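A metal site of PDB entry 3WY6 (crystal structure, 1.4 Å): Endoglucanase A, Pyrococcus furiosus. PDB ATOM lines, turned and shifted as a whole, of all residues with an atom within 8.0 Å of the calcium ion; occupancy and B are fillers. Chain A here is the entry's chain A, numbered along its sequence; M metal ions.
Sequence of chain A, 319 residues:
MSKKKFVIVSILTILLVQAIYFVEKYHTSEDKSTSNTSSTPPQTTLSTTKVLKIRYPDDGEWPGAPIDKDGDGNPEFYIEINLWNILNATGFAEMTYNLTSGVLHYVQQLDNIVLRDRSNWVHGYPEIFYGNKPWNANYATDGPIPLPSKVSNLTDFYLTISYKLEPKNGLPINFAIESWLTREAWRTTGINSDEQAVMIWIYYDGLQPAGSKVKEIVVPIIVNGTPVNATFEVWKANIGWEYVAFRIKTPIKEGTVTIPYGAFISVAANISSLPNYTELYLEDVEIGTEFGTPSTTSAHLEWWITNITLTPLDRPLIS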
ATOM      1  N   ILE A  67     -30.275   0.195  17.729  1.00  0.00           N
ATOM      2  CA  ILE A  67     -29.258   1.171  18.153  1.00  0.00           C
ATOM      3  C   ILE A  67     -28.241   0.332  18.878  1.00  0.00           C
ATOM      4  O   ILE A  67     -28.519  -0.253  19.924  1.00  0.00           O
ATOM      5  CB  ILE A  67     -29.823   2.279  19.037  1.00  0.00           C
ATOM      6  CG1 ILE A  67     -30.775   3.150  18.140  1.00  0.00           C
ATOM      7  CG2 ILE A  67     -28.674   3.086  19.682  1.00  0.00           C
ATOM      8  CD1 ILE A  67     -31.510   4.125  18.966  1.00  0.00           C
ATOM      9  N   ASP A  68     -27.042   0.214  18.272  1.00  0.00           N
ATOM     10  CA  ASP A  68     -26.010  -0.684  18.806  1.00  0.00           C
ATOM     11  C   ASP A  68     -24.699   0.099  18.769  1.00  0.00           C
ATOM     12  O   ASP A  68     -23.838  -0.075  17.821  1.00  0.00           O
ATOM     13  CB  ASP A  68     -25.976  -1.958  17.933  1.00  0.00           C
ATOM     14  CG  ASP A  68     -24.946  -2.982  18.437  1.00  0.00           C
ATOM     15  OD1 ASP A  68     -24.462  -2.909  19.593  1.00  0.00           O
ATOM     16  OD2 ASP A  68     -24.599  -3.913  17.652  1.00  0.00           O
ATOM     17  N   LYS A  69     -24.471   0.950  19.790  1.00  0.00           N
ATOM     18  CA  LYS A  69     -23.404   1.941  19.677  1.00  0.00           C
ATOM     19  C   LYS A  69     -22.012   1.316  19.740  1.00  0.00           C
ATOM     20  O   LYS A  69     -21.059   1.867  19.135  1.00  0.00           O
ATOM     21  CB  LYS A  69     -23.536   3.004  20.763  1.00  0.00           C
ATOM     22  CG  LYS A  69     -22.579   4.195  20.599  1.00  0.00           C
ATOM     23  CD  LYS A  69     -22.600   5.197  21.754  1.00  0.00           C
ATOM     24  CE  LYS A  69     -21.283   5.945  21.857  1.00  0.00           C
ATOM     25  NZ  LYS A  69     -21.292   6.902  20.743  1.00  0.00           N
ATOM     26  N   ASP A  70     -21.874   0.213  20.464  1.00  0.00           N
ATOM     27  CA  ASP A  70     -20.571  -0.483  20.577  1.00  0.00           C
ATOM     28  C   ASP A  70     -20.438  -1.520  19.452  1.00  0.00           C
ATOM     29  O   ASP A  70     -19.435  -2.200  19.369  1.00  0.00           O
ATOM     30  CB  ASP A  70     -20.335  -1.024  21.987  1.00  0.00           C
ATOM     31  CG  ASP A  70     -21.366  -2.048  22.424  1.00  0.00           C
ATOM     32  OD1 ASP A  70     -22.408  -2.200  21.745  1.00  0.00           O
ATOM     33  OD2 ASP A  70     -21.127  -2.730  23.473  1.00  0.00           O
ATOM     34  N   GLY A  71     -21.424  -1.628  18.558  1.00  0.00           N
ATOM     35  CA  GLY A  71     -21.352  -2.603  17.440  1.00  0.00           C
ATOM     36  C   GLY A  71     -21.160  -4.055  17.913  1.00  0.00           C
ATOM     37  O   GLY A  71     -20.522  -4.849  17.159  1.00  0.00           O
ATOM     38  N   ASP A  72     -21.703  -4.439  19.061  1.00  0.00           N
ATOM     39  CA  ASP A  72     -21.463  -5.803  19.588  1.00  0.00           C
ATOM     40  C   ASP A  72     -22.576  -6.806  19.273  1.00  0.00           C
ATOM     41  O   ASP A  72     -22.526  -7.976  19.741  1.00  0.00           O
ATOM     42  CB  ASP A  72     -21.132  -5.805  21.103  1.00  0.00           C
ATOM     43  CG  ASP A  72     -22.387  -5.612  22.005  1.00  0.00           C
ATOM     44  OD1 ASP A  72     -23.469  -5.249  21.479  1.00  0.00           O
ATOM     45  OD2 ASP A  72     -22.247  -5.846  23.227  1.00  0.00           O
ATOM     46  N   GLY A  73     -23.553  -6.392  18.455  1.00  0.00           N
ATOM     47  CA  GLY A  73     -24.607  -7.315  18.012  1.00  0.00           C
ATOM     48  C   GLY A  73     -25.778  -7.476  18.997  1.00  0.00           C
ATOM     49  O   GLY A  73     -26.715  -8.277  18.717  1.00  0.00           O
ATOM     50  N   ASN A  74     -25.751  -6.725  20.152  1.00  0.00           N
ATOM     51  CA  ASN A  74     -26.844  -6.719  21.154  1.00  0.00           C
ATOM     52  C   ASN A  74     -27.247  -5.228  21.262  1.00  0.00           C
ATOM     53  O   ASN A  74     -26.474  -4.388  21.708  1.00  0.00           O
ATOM     54  CB  ASN A  74     -26.350  -7.228  22.475  1.00  0.00           C
ATOM     55  CG  ASN A  74     -27.489  -7.450  23.448  1.00  0.00           C
ATOM     56  OD1 ASN A  74     -28.653  -7.317  23.069  1.00  0.00           O
ATOM     57  ND2 ASN A  74     -27.167  -7.802  24.692  1.00  0.00           N
ATOM     58  N   PRO A  75     -28.378  -4.876  20.673  1.00  0.00           N
ATOM     59  CA  PRO A  75     -28.728  -3.404  20.635  1.00  0.00           C
ATOM     60  C   PRO A  75     -28.979  -2.888  22.101  1.00  0.00           C
ATOM     61  O   PRO A  75     -29.485  -3.656  22.966  1.00  0.00           O
ATOM     62  CB  PRO A  75     -30.064  -3.386  19.856  1.00  0.00           C
ATOM     63  CG  PRO A  75     -30.020  -4.689  18.980  1.00  0.00           C
ATOM     64  CD  PRO A  75     -29.378  -5.703  19.929  1.00  0.00           C
ATOM     65  N   GLU A  76     -28.607  -1.641  22.368  1.00  0.00           N
ATOM     66  CA  GLU A  76     -29.033  -1.001  23.574  1.00  0.00           C
ATOM     67  C   GLU A  76     -30.536  -0.593  23.545  1.00  0.00           C
ATOM     68  O   GLU A  76     -31.199  -0.594  24.616  1.00  0.00           O
ATOM     69  CB  GLU A  76     -28.217   0.259  23.864  1.00  0.00           C
ATOM     70  CG  GLU A  76     -26.703  -0.028  23.991  1.00  0.00           C
ATOM     71  CD  GLU A  76     -25.984   0.015  22.646  1.00  0.00           C
ATOM     72  OE1 GLU A  76     -26.077   1.038  21.915  1.00  0.00           O
ATOM     73  OE2 GLU A  76     -25.279  -0.973  22.309  1.00  0.00           O
ATOM     74  N   PHE A  77     -31.050  -0.202  22.366  1.00  0.00           N
ATOM     75  CA  PHE A  77     -32.474   0.143  22.202  1.00  0.00           C
ATOM     76  C   PHE A  77     -32.797  -0.247  20.763  1.00  0.00           C
ATOM     77  O   PHE A  77     -31.911  -0.500  19.938  1.00  0.00           O
ATOM     78  CB  PHE A  77     -32.690   1.679  22.333  1.00  0.00           C
ATOM     79  CG  PHE A  77     -32.401   2.178  23.734  1.00  0.00           C
ATOM     80  CD1 PHE A  77     -33.374   2.061  24.701  1.00  0.00           C
ATOM     81  CD2 PHE A  77     -31.185   2.777  24.069  1.00  0.00           C
ATOM     82  CE1 PHE A  77     -33.137   2.411  26.020  1.00  0.00           C
ATOM     83  CE2 PHE A  77     -30.964   3.195  25.390  1.00  0.00           C
ATOM     84  CZ  PHE A  77     -31.932   2.982  26.377  1.00  0.00           C
ATOM     85  N   THR A 141     -31.196  -5.858  24.289  1.00  0.00           N
ATOM     86  CA  THR A 141     -30.996  -6.324  25.678  1.00  0.00           C
ATOM     87  C   THR A 141     -29.669  -5.906  26.271  1.00  0.00           C
ATOM     88  O   THR A 141     -29.275  -6.413  27.324  1.00  0.00           O
ATOM     89  CB  THR A 141     -31.212  -7.867  25.797  1.00  0.00           C
ATOM     90  OG1 THR A 141     -30.214  -8.537  25.035  1.00  0.00           O
ATOM     91  CG2 THR A 141     -32.654  -8.329  25.408  1.00  0.00           C
ATOM     92  N   ASP A 142     -28.994  -4.920  25.656  1.00  0.00           N
ATOM     93  CA  ASP A 142     -27.700  -4.455  26.193  1.00  0.00           C
ATOM     94  C   ASP A 142     -28.015  -3.294  27.144  1.00  0.00           C
ATOM     95  O   ASP A 142     -28.016  -2.108  26.703  1.00  0.00           O
ATOM     96  CB  ASP A 142     -26.856  -3.993  24.972  1.00  0.00           C
ATOM     97  CG  ASP A 142     -25.391  -3.644  25.302  1.00  0.00           C
ATOM     98  OD1 ASP A 142     -25.025  -3.585  26.483  1.00  0.00           O
ATOM     99  OD2 ASP A 142     -24.616  -3.492  24.310  1.00  0.00           O
ATOM    100  N   GLY A 143     -28.313  -3.619  28.395  1.00  0.00           N
ATOM    101  CA  GLY A 143     -28.711  -2.638  29.428  1.00  0.00           C
ATOM    102  C   GLY A 143     -28.671  -3.268  30.791  1.00  0.00           C
ATOM    103  O   GLY A 143     -28.516  -4.501  30.909  1.00  0.00           O
HETATM  104 CA    CA M   1     -24.540  -3.147  21.957  1.00  0.00          CA
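The backbone carbonyl oxygen of Pro 75 is in hydrogen-bond range of the backbone NH of Asp 142, at 3.0 Å.
OD1 of Asp 68 lies close to N of Gly 71 (3.5 Å).
N of Glu 76 sits at hydrogen-bond distance from O of Ile 67 (2.8 Å).
The side-chain carboxylate (OD2) of Asp 68 lies within hydrogen-bond range of the backbone NH (N) of Gly 73, at 2.8 Å.
The side-chain amide oxygen (OD1) of Asn 74 lies within hydrogen-bond range of the side-chain hydroxyl (OG1) of Thr 141.
The side-chain carboxylate of Glu 76 sits at hydrogen-bond distance from the backbone NH of Lys 69 (2.7 Å).
Six residues have an atom within 4 Å of the calcium ion: Asp 68, Asp 70, Asp 72, Asn 74, Glu 76 and Asp 142.
The nearest printed residue that does not touch the calcium ion is Pro 75 (4.4 Å).
The calcium ion is bound by O of Asn 74, OE2 of Glu 76, OD1 of Asp 70, OD1 of Asp 68, OD2 of Asp 142 and OD1 of Asp 72.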
